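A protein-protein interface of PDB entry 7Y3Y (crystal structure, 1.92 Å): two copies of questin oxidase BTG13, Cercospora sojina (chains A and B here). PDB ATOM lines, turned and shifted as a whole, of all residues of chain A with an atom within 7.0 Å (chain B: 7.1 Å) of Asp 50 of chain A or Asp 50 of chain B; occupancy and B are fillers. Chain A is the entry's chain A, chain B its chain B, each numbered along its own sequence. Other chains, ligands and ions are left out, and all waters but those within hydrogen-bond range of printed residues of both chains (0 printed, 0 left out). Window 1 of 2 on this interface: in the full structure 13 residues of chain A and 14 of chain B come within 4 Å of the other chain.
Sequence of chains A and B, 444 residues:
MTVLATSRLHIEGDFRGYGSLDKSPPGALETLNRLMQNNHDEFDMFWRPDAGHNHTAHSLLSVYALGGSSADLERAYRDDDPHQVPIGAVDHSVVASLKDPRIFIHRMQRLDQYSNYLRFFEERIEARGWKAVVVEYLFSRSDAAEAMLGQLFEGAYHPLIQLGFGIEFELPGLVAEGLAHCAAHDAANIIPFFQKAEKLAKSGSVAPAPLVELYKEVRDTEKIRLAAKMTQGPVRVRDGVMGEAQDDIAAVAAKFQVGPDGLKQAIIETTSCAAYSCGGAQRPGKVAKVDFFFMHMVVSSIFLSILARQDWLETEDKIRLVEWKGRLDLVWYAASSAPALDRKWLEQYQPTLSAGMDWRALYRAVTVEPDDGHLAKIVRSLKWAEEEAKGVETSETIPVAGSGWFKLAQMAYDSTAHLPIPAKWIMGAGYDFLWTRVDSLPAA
Of the printed residues of chain B, Trp 47 of chain A touches Thr 231. Of the printed residues of chain A, Trp 47 of chain B touches Thr 231. Printed residues of chain A within 4 Å of Arg 48 of chain B: Thr 231 (3.8 Å). Of chain A, only Asp 50 (3.6 Å) comes within 4 Å of Asp 50 of chain B. Ala 51 of chain B touches none of the printed residues of chain A. Leu 111 of chain B touches none of the printed residues of chain A. Of the printed residues of chain A, Thr 231 of chain B touches Trp 47, Arg 48 and Pro 49. The nearest residue of chain B that does not touch Asp 50 of chain A is Pro 49 of chain B (6.0 Å).
Of the 13 printed residues of chain A, 5 touch a printed residue of chain B. Printed residues of chain A that touch a printed residue of chain B: Trp 47, Arg 48, Pro 49, Asp 50 and Thr 231. Hydrophobic or aromatic side chains of chain A that line the printed part of chain B: Pro 49. Hydrophobic or aromatic side chains of chain B that line the printed part of chain A: Pro 49. Among the printed residues, no Asp or Glu carboxylate lies within 4 Å of a Lys or Arg side-chain nitrogen of the other chain.
Among the printed residues, pairs that only touch across the chains: Pro 49 of chain A with Thr 231 of chain B (3.4 Å), Thr 231 of chain A with Pro 49 of chain B (3.4 Å), Asp 50 of chain A with Asp 50 of chain B (3.6 Å), Thr 231 of chain A with Trp 47 of chain B (3.6 Å), Arg 48 of chain A with Thr 231 of chain B (3.7 Å), Thr 231 of chain A with Arg 48 of chain B (3.8 Å) and Trp 47 of chain A with Thr 231 of chain B (3.8 Å).
The backbone carbonyl oxygen of His 53 of chain A sits at hydrogen-bond distance from the indole nitrogen of Trp 47 of chain A (3.1 Å). The guanidinium group of Arg 48 of chain A lies within hydrogen-bond range of the backbone carbonyl oxygen of Ala 51 of chain A (3.0 Å). O of Gly 52 of chain B sits at hydrogen-bond distance from N of Trp 47 of chain B, 2.8 Å away. NE1 of Trp 47 of chain B lies within hydrogen-bond range of O of His 53 of chain B (3.2 Å). The backbone carbonyl oxygen (O) of Asp 50 of chain B lies within hydrogen-bond range of the guanidinium group (NE) of Arg 48 of chain B, at 3.1 Å. NH2 of Arg 48 of chain B lies within hydrogen-bond range of O of Ala 51 of chain B, at 3.2 Å.
Trp 47 of chain A touches Thr 231 of chain B, and with the chains exchanged Thr 231 of chain A touches Trp 47 of chain B. Arg 48 of chain A touches Thr 231 of chain B, and with the chains exchanged Thr 231 of chain A touches Arg 48 of chain B. Pro 49 of chain A touches Thr 231 of chain B, and with the chains exchanged Thr 231 of chain A touches Pro 49 of chain B. Asp 50 of chain A touches its own counterpart, Asp 50 of chain B. Positions printed for both chains: 47, 48, 49, 50, 51, 52, 53, 111, 186, 231, 234, 235 and 238. Of the 7 pairs that touch across the chains among the printed residues, 7 have their exchanged pair printed and touching as well.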
ATOM      1  N   TRP A  47     -11.146 -13.863  21.185  1.00  0.00           N
ATOM      2  CA  TRP A  47     -12.145 -14.827  21.714  1.00  0.00           C
ATOM      3  C   TRP A  47     -13.511 -14.169  21.970  1.00  0.00           C
ATOM      4  O   TRP A  47     -14.458 -14.923  22.304  1.00  0.00           O
ATOM      5  CB  TRP A  47     -11.618 -15.560  22.943  1.00  0.00           C
ATOM      6  CG  TRP A  47     -11.104 -14.705  24.065  1.00  0.00           C
ATOM      7  CD1 TRP A  47      -9.827 -14.243  24.222  1.00  0.00           C
ATOM      8  CD2 TRP A  47     -11.812 -14.314  25.251  1.00  0.00           C
ATOM      9  NE1 TRP A  47      -9.720 -13.509  25.373  1.00  0.00           N
ATOM     10  CE2 TRP A  47     -10.911 -13.566  26.050  1.00  0.00           C
ATOM     11  CE3 TRP A  47     -13.105 -14.532  25.726  1.00  0.00           C
ATOM     12  CZ2 TRP A  47     -11.260 -13.048  27.298  1.00  0.00           C
ATOM     13  CZ3 TRP A  47     -13.470 -13.972  26.930  1.00  0.00           C
ATOM     14  CH2 TRP A  47     -12.547 -13.263  27.715  1.00  0.00           C
ATOM     15  N   ARG A  48     -13.634 -12.844  21.791  1.00  0.00           N
ATOM     16  CA  ARG A  48     -14.930 -12.112  21.832  1.00  0.00           C
ATOM     17  C   ARG A  48     -14.699 -10.725  21.252  1.00  0.00           C
ATOM     18  O   ARG A  48     -13.567 -10.319  21.064  1.00  0.00           O
ATOM     19  CB  ARG A  48     -15.506 -12.041  23.254  1.00  0.00           C
ATOM     20  CG  ARG A  48     -14.558 -11.389  24.255  1.00  0.00           C
ATOM     21  CD  ARG A  48     -15.188 -10.997  25.581  1.00  0.00           C
ATOM     22  NE  ARG A  48     -14.204 -10.380  26.473  1.00  0.00           N
ATOM     23  CZ  ARG A  48     -14.309 -10.334  27.793  1.00  0.00           C
ATOM     24  NH1 ARG A  48     -15.359 -10.845  28.412  1.00  0.00           N
ATOM     25  NH2 ARG A  48     -13.346  -9.792  28.504  1.00  0.00           N
ATOM     26  N   PRO A  49     -15.754  -9.986  20.848  1.00  0.00           N
ATOM     27  CA  PRO A  49     -15.550  -8.785  20.024  1.00  0.00           C
ATOM     28  C   PRO A  49     -14.872  -7.585  20.710  1.00  0.00           C
ATOM     29  O   PRO A  49     -14.278  -6.752  19.999  1.00  0.00           O
ATOM     30  CB  PRO A  49     -16.970  -8.379  19.575  1.00  0.00           C
ATOM     31  CG  PRO A  49     -17.829  -9.565  19.880  1.00  0.00           C
ATOM     32  CD  PRO A  49     -17.165 -10.369  20.978  1.00  0.00           C
ATOM     33  N   ASP A  50     -15.027  -7.481  22.019  1.00  0.00           N
ATOM     34  CA  ASP A  50     -14.496  -6.370  22.855  1.00  0.00           C
ATOM     35  C   ASP A  50     -13.708  -6.995  24.022  1.00  0.00           C
ATOM     36  O   ASP A  50     -14.208  -7.919  24.690  1.00  0.00           O
ATOM     37  CB  ASP A  50     -15.614  -5.445  23.380  1.00  0.00           C
ATOM     38  CG  ASP A  50     -16.432  -4.711  22.320  1.00  0.00           C
ATOM     39  OD1 ASP A  50     -15.820  -4.040  21.448  1.00  0.00           O
ATOM     40  OD2 ASP A  50     -17.671  -4.807  22.364  1.00  0.00           O
ATOM     41  N   ALA A  51     -12.531  -6.466  24.298  1.00  0.00           N
ATOM     42  CA  ALA A  51     -11.663  -6.910  25.414  1.00  0.00           C
ATOM     43  C   ALA A  51     -11.416  -8.419  25.292  1.00  0.00           C
ATOM     44  O   ALA A  51     -11.461  -9.149  26.324  1.00  0.00           O
ATOM     45  CB  ALA A  51     -12.311  -6.550  26.725  1.00  0.00           C
ATOM     46  N   GLY A  52     -11.204  -8.897  24.062  1.00  0.00           N
ATOM     47  CA  GLY A  52     -11.186 -10.338  23.777  1.00  0.00           C
ATOM     48  C   GLY A  52      -9.836 -10.799  23.289  1.00  0.00           C
ATOM     49  O   GLY A  52      -9.792 -11.705  22.461  1.00  0.00           O
ATOM     50  N   HIS A  53      -8.748 -10.214  23.773  1.00  0.00           N
ATOM     51  CA  HIS A  53      -7.398 -10.544  23.261  1.00  0.00           C
ATOM     52  C   HIS A  53      -6.914 -11.813  23.970  1.00  0.00           C
ATOM     53  O   HIS A  53      -7.101 -11.933  25.226  1.00  0.00           O
ATOM     54  CB  HIS A  53      -6.439  -9.364  23.443  1.00  0.00           C
ATOM     55  CG  HIS A  53      -6.978  -8.031  23.033  1.00  0.00           C
ATOM     56  ND1 HIS A  53      -7.698  -7.228  23.905  1.00  0.00           N
ATOM     57  CD2 HIS A  53      -6.821  -7.309  21.896  1.00  0.00           C
ATOM     58  CE1 HIS A  53      -7.976  -6.095  23.313  1.00  0.00           C
ATOM     59  NE2 HIS A  53      -7.449  -6.111  22.073  1.00  0.00           N
ATOM     60  N   LEU A 111     -11.855  -8.528  12.815  1.00  0.00           N
ATOM     61  CA  LEU A 111     -11.290  -9.571  13.724  1.00  0.00           C
ATOM     62  C   LEU A 111     -11.223 -10.937  13.042  1.00  0.00           C
ATOM     63  O   LEU A 111     -10.305 -11.702  13.352  1.00  0.00           O
ATOM     64  CB  LEU A 111     -12.167  -9.667  14.975  1.00  0.00           C
ATOM     65  CG  LEU A 111     -12.248  -8.395  15.824  1.00  0.00           C
ATOM     66  CD1 LEU A 111     -13.067  -8.683  17.060  1.00  0.00           C
ATOM     67  CD2 LEU A 111     -10.851  -7.882  16.209  1.00  0.00           C
ATOM     68  N   ASP A 186     -10.138  -4.484  15.469  1.00  0.00           N
ATOM     69  CA  ASP A 186     -11.250  -3.542  15.184  1.00  0.00           C
ATOM     70  C   ASP A 186     -10.774  -2.131  15.536  1.00  0.00           C
ATOM     71  O   ASP A 186      -9.872  -1.998  16.424  1.00  0.00           O
ATOM     72  CB  ASP A 186     -12.531  -3.915  15.942  1.00  0.00           C
ATOM     73  CG  ASP A 186     -12.325  -3.889  17.437  1.00  0.00           C
ATOM     74  OD1 ASP A 186     -11.528  -4.705  17.920  1.00  0.00           O
ATOM     75  OD2 ASP A 186     -12.877  -2.991  18.082  1.00  0.00           O
ATOM     76  N   THR A 231     -20.487   3.480  31.523  1.00  0.00           N
ATOM     77  CA  THR A 231     -21.170   2.279  30.965  1.00  0.00           C
ATOM     78  C   THR A 231     -20.878   2.133  29.473  1.00  0.00           C
ATOM     79  O   THR A 231     -21.439   1.210  28.882  1.00  0.00           O
ATOM     80  CB  THR A 231     -22.670   2.274  31.280  1.00  0.00           C
ATOM     81  OG1 THR A 231     -23.192   3.452  30.703  1.00  0.00           O
ATOM     82  CG2 THR A 231     -22.931   2.176  32.771  1.00  0.00           C
ATOM     83  N   PRO A 234     -15.869  -1.239  27.359  1.00  0.00           N
ATOM     84  CA  PRO A 234     -14.739  -1.395  26.427  1.00  0.00           C
ATOM     85  C   PRO A 234     -14.724  -0.403  25.246  1.00  0.00           C
ATOM     86  O   PRO A 234     -13.704  -0.302  24.559  1.00  0.00           O
ATOM     87  CB  PRO A 234     -14.915  -2.842  25.941  1.00  0.00           C
ATOM     88  CG  PRO A 234     -16.442  -3.029  25.923  1.00  0.00           C
ATOM     89  CD  PRO A 234     -16.845  -2.343  27.220  1.00  0.00           C
ATOM     90  N   VAL A 235     -15.793   0.359  25.020  1.00  0.00           N
ATOM     91  CA  VAL A 235     -15.871   1.288  23.864  1.00  0.00           C
ATOM     92  C   VAL A 235     -15.929   2.747  24.324  1.00  0.00           C
ATOM     93  O   VAL A 235     -16.349   3.587  23.541  1.00  0.00           O
ATOM     94  CB  VAL A 235     -17.010   0.875  22.907  1.00  0.00           C
ATOM     95  CG1 VAL A 235     -16.742  -0.533  22.386  1.00  0.00           C
ATOM     96  CG2 VAL A 235     -18.392   0.949  23.527  1.00  0.00           C
ATOM     97  N   ARG A 238     -13.618   4.652  21.554  1.00  0.00           N
ATOM     98  CA  ARG A 238     -14.285   4.836  20.245  1.00  0.00           C
ATOM     99  C   ARG A 238     -15.469   5.808  20.408  1.00  0.00           C
ATOM    100  O   ARG A 238     -15.524   6.835  19.670  1.00  0.00           O
ATOM    101  CB  ARG A 238     -14.685   3.493  19.631  1.00  0.00           C
ATOM    102  CG  ARG A 238     -15.364   3.627  18.273  1.00  0.00           C
ATOM    103  CD  ARG A 238     -15.959   2.320  17.820  1.00  0.00           C
ATOM    104  NE  ARG A 238     -17.146   1.983  18.577  1.00  0.00           N
ATOM    105  CZ  ARG A 238     -17.559   0.743  18.852  1.00  0.00           C
ATOM    106  NH1 ARG A 238     -16.913  -0.335  18.417  1.00  0.00           N
ATOM    107  NH2 ARG A 238     -18.634   0.601  19.599  1.00  0.00           N
ATOM    108  N   TRP B  47     -26.389  -1.353  31.827  1.00  0.00           N
ATOM    109  CA  TRP B  47     -25.178  -1.268  32.677  1.00  0.00           C
ATOM    110  C   TRP B  47     -23.909  -1.618  31.880  1.00  0.00           C
ATOM    111  O   TRP B  47     -22.825  -1.424  32.417  1.00  0.00           O
ATOM    112  CB  TRP B  47     -25.365  -2.133  33.913  1.00  0.00           C
ATOM    113  CG  TRP B  47     -25.715  -3.567  33.681  1.00  0.00           C
ATOM    114  CD1 TRP B  47     -26.956  -4.113  33.523  1.00  0.00           C
ATOM    115  CD2 TRP B  47     -24.788  -4.658  33.649  1.00  0.00           C
ATOM    116  NE1 TRP B  47     -26.860  -5.472  33.356  1.00  0.00           N
ATOM    117  CE2 TRP B  47     -25.542  -5.834  33.441  1.00  0.00           C
ATOM    118  CE3 TRP B  47     -23.399  -4.751  33.801  1.00  0.00           C
ATOM    119  CZ2 TRP B  47     -24.941  -7.096  33.393  1.00  0.00           C
ATOM    120  CZ3 TRP B  47     -22.800  -5.993  33.723  1.00  0.00           C
ATOM    121  CH2 TRP B  47     -23.567  -7.145  33.530  1.00  0.00           C
ATOM    122  N   ARG B  48     -24.029  -2.037  30.624  1.00  0.00           N
ATOM    123  CA  ARG B  48     -22.869  -2.177  29.706  1.00  0.00           C
ATOM    124  C   ARG B  48     -23.389  -2.218  28.276  1.00  0.00           C
ATOM    125  O   ARG B  48     -24.574  -2.386  28.049  1.00  0.00           O
ATOM    126  CB  ARG B  48     -22.066  -3.441  30.028  1.00  0.00           C
ATOM    127  CG  ARG B  48     -22.851  -4.738  29.894  1.00  0.00           C
ATOM    128  CD  ARG B  48     -21.984  -5.991  30.074  1.00  0.00           C
ATOM    129  NE  ARG B  48     -22.808  -7.182  30.125  1.00  0.00           N
ATOM    130  CZ  ARG B  48     -22.449  -8.362  30.653  1.00  0.00           C
ATOM    131  NH1 ARG B  48     -21.260  -8.520  31.211  1.00  0.00           N
ATOM    132  NH2 ARG B  48     -23.307  -9.368  30.657  1.00  0.00           N
ATOM    133  N   PRO B  49     -22.533  -2.009  27.252  1.00  0.00           N
ATOM    134  CA  PRO B  49     -23.023  -1.803  25.882  1.00  0.00           C
ATOM    135  C   PRO B  49     -23.697  -3.025  25.231  1.00  0.00           C
ATOM    136  O   PRO B  49     -24.572  -2.836  24.379  1.00  0.00           O
ATOM    137  CB  PRO B  49     -21.781  -1.380  25.081  1.00  0.00           C
ATOM    138  CG  PRO B  49     -20.738  -1.055  26.142  1.00  0.00           C
ATOM    139  CD  PRO B  49     -21.079  -1.864  27.372  1.00  0.00           C
ATOM    140  N   ASP B  50     -23.269  -4.225  25.611  1.00  0.00           N
ATOM    141  CA  ASP B  50     -23.788  -5.501  25.057  1.00  0.00           C
ATOM    142  C   ASP B  50     -24.199  -6.404  26.221  1.00  0.00           C
ATOM    143  O   ASP B  50     -23.420  -6.521  27.202  1.00  0.00           O
ATOM    144  CB  ASP B  50     -22.761  -6.225  24.171  1.00  0.00           C
ATOM    145  CG  ASP B  50     -22.375  -5.459  22.908  1.00  0.00           C
ATOM    146  OD1 ASP B  50     -23.278  -5.125  22.070  1.00  0.00           O
ATOM    147  OD2 ASP B  50     -21.196  -5.219  22.761  1.00  0.00           O
ATOM    148  N   ALA B  51     -25.391  -6.996  26.095  1.00  0.00           N
ATOM    149  CA  ALA B  51     -25.995  -7.915  27.086  1.00  0.00           C
ATOM    150  C   ALA B  51     -26.034  -7.235  28.475  1.00  0.00           C
ATOM    151  O   ALA B  51     -25.842  -7.896  29.483  1.00  0.00           O
ATOM    152  CB  ALA B  51     -25.236  -9.213  27.063  1.00  0.00           C
ATOM    153  N   GLY B  52     -26.366  -5.950  28.533  1.00  0.00           N
ATOM    154  CA  GLY B  52     -26.324  -5.173  29.782  1.00  0.00           C
ATOM    155  C   GLY B  52     -27.695  -4.679  30.197  1.00  0.00           C
ATOM    156  O   GLY B  52     -27.782  -3.560  30.719  1.00  0.00           O
ATOM    157  N   HIS B  53     -28.736  -5.485  30.021  1.00  0.00           N
ATOM    158  CA  HIS B  53     -30.114  -5.141  30.469  1.00  0.00           C
ATOM    159  C   HIS B  53     -30.229  -5.329  31.979  1.00  0.00           C
ATOM    160  O   HIS B  53     -29.775  -6.372  32.482  1.00  0.00           O
ATOM    161  CB  HIS B  53     -31.159  -6.003  29.748  1.00  0.00           C
ATOM    162  CG  HIS B  53     -30.903  -6.099  28.293  1.00  0.00           C
ATOM    163  ND1 HIS B  53     -30.029  -7.038  27.766  1.00  0.00           N
ATOM    164  CD2 HIS B  53     -31.404  -5.391  27.249  1.00  0.00           C
ATOM    165  CE1 HIS B  53     -29.998  -6.885  26.453  1.00  0.00           C
ATOM    166  NE2 HIS B  53     -30.840  -5.884  26.110  1.00  0.00           N
ATOM    167  N   LEU B 111     -28.600   3.957  23.681  1.00  0.00           N
ATOM    168  CA  LEU B 111     -28.727   3.493  25.085  1.00  0.00           C
ATOM    169  C   LEU B 111     -28.759   4.670  26.078  1.00  0.00           C
ATOM    170  O   LEU B 111     -29.487   4.597  27.106  1.00  0.00           O
ATOM    171  CB  LEU B 111     -27.533   2.571  25.388  1.00  0.00           C
ATOM    172  CG  LEU B 111     -27.466   1.276  24.577  1.00  0.00           C
ATOM    173  CD1 LEU B 111     -26.351   0.352  25.100  1.00  0.00           C
ATOM    174  CD2 LEU B 111     -28.792   0.535  24.608  1.00  0.00           C
ATOM    175  N   ASP B 186     -30.138  -0.285  21.483  1.00  0.00           N
ATOM    176  CA  ASP B 186     -29.241  -0.260  20.286  1.00  0.00           C
ATOM    177  C   ASP B 186     -29.830  -1.249  19.268  1.00  0.00           C
ATOM    178  O   ASP B 186     -30.508  -2.211  19.704  1.00  0.00           O
ATOM    179  CB  ASP B 186     -27.790  -0.545  20.680  1.00  0.00           C
ATOM    180  CG  ASP B 186     -27.627  -1.950  21.237  1.00  0.00           C
ATOM    181  OD1 ASP B 186     -28.270  -2.248  22.267  1.00  0.00           O
ATOM    182  OD2 ASP B 186     -27.004  -2.776  20.555  1.00  0.00           O
ATOM    183  N   THR B 231     -17.537 -16.434  17.998  1.00  0.00           N
ATOM    184  CA  THR B 231     -16.798 -15.334  18.680  1.00  0.00           C
ATOM    185  C   THR B 231     -17.378 -13.956  18.314  1.00  0.00           C
ATOM    186  O   THR B 231     -16.829 -12.923  18.812  1.00  0.00           O
ATOM    187  CB  THR B 231     -15.296 -15.410  18.405  1.00  0.00           C
ATOM    188  OG1 THR B 231     -15.146 -15.234  17.000  1.00  0.00           O
ATOM    189  CG2 THR B 231     -14.689 -16.678  18.935  1.00  0.00           C
ATOM    190  N   PRO B 234     -22.251 -11.388  21.643  1.00  0.00           N
ATOM    191  CA  PRO B 234     -23.526 -10.650  21.722  1.00  0.00           C
ATOM    192  C   PRO B 234     -23.963  -9.943  20.423  1.00  0.00           C
ATOM    193  O   PRO B 234     -25.092  -9.524  20.388  1.00  0.00           O
ATOM    194  CB  PRO B 234     -23.296  -9.654  22.891  1.00  0.00           C
ATOM    195  CG  PRO B 234     -21.783  -9.425  22.892  1.00  0.00           C
ATOM    196  CD  PRO B 234     -21.171 -10.727  22.408  1.00  0.00           C
ATOM    197  N   VAL B 235     -23.138  -9.937  19.360  1.00  0.00           N
ATOM    198  CA  VAL B 235     -23.471  -9.239  18.080  1.00  0.00           C
ATOM    199  C   VAL B 235     -23.589 -10.254  16.936  1.00  0.00           C
ATOM    200  O   VAL B 235     -23.464  -9.848  15.786  1.00  0.00           O
ATOM    201  CB  VAL B 235     -22.491  -8.083  17.779  1.00  0.00           C
ATOM    202  CG1 VAL B 235     -22.555  -7.000  18.868  1.00  0.00           C
ATOM    203  CG2 VAL B 235     -21.068  -8.567  17.569  1.00  0.00           C
ATOM    204  N   ARG B 238     -26.747  -9.060  14.708  1.00  0.00           N
ATOM    205  CA  ARG B 238     -26.447  -7.856  13.918  1.00  0.00           C
ATOM    206  C   ARG B 238     -25.425  -8.222  12.832  1.00  0.00           C
ATOM    207  O   ARG B 238     -25.777  -8.071  11.667  1.00  0.00           O
ATOM    208  CB  ARG B 238     -25.950  -6.722  14.817  1.00  0.00           C
ATOM    209  CG  ARG B 238     -25.707  -5.418  14.066  1.00  0.00           C
ATOM    210  CD  ARG B 238     -25.015  -4.401  14.941  1.00  0.00           C
ATOM    211  NE  ARG B 238     -23.629  -4.773  15.199  1.00  0.00           N
ATOM    212  CZ  ARG B 238     -22.934  -4.439  16.287  1.00  0.00           C
ATOM    213  NH1 ARG B 238     -23.463  -3.707  17.258  1.00  0.00           N
ATOM    214  NH2 ARG B 238     -21.688  -4.853  16.407  1.00  0.00           N
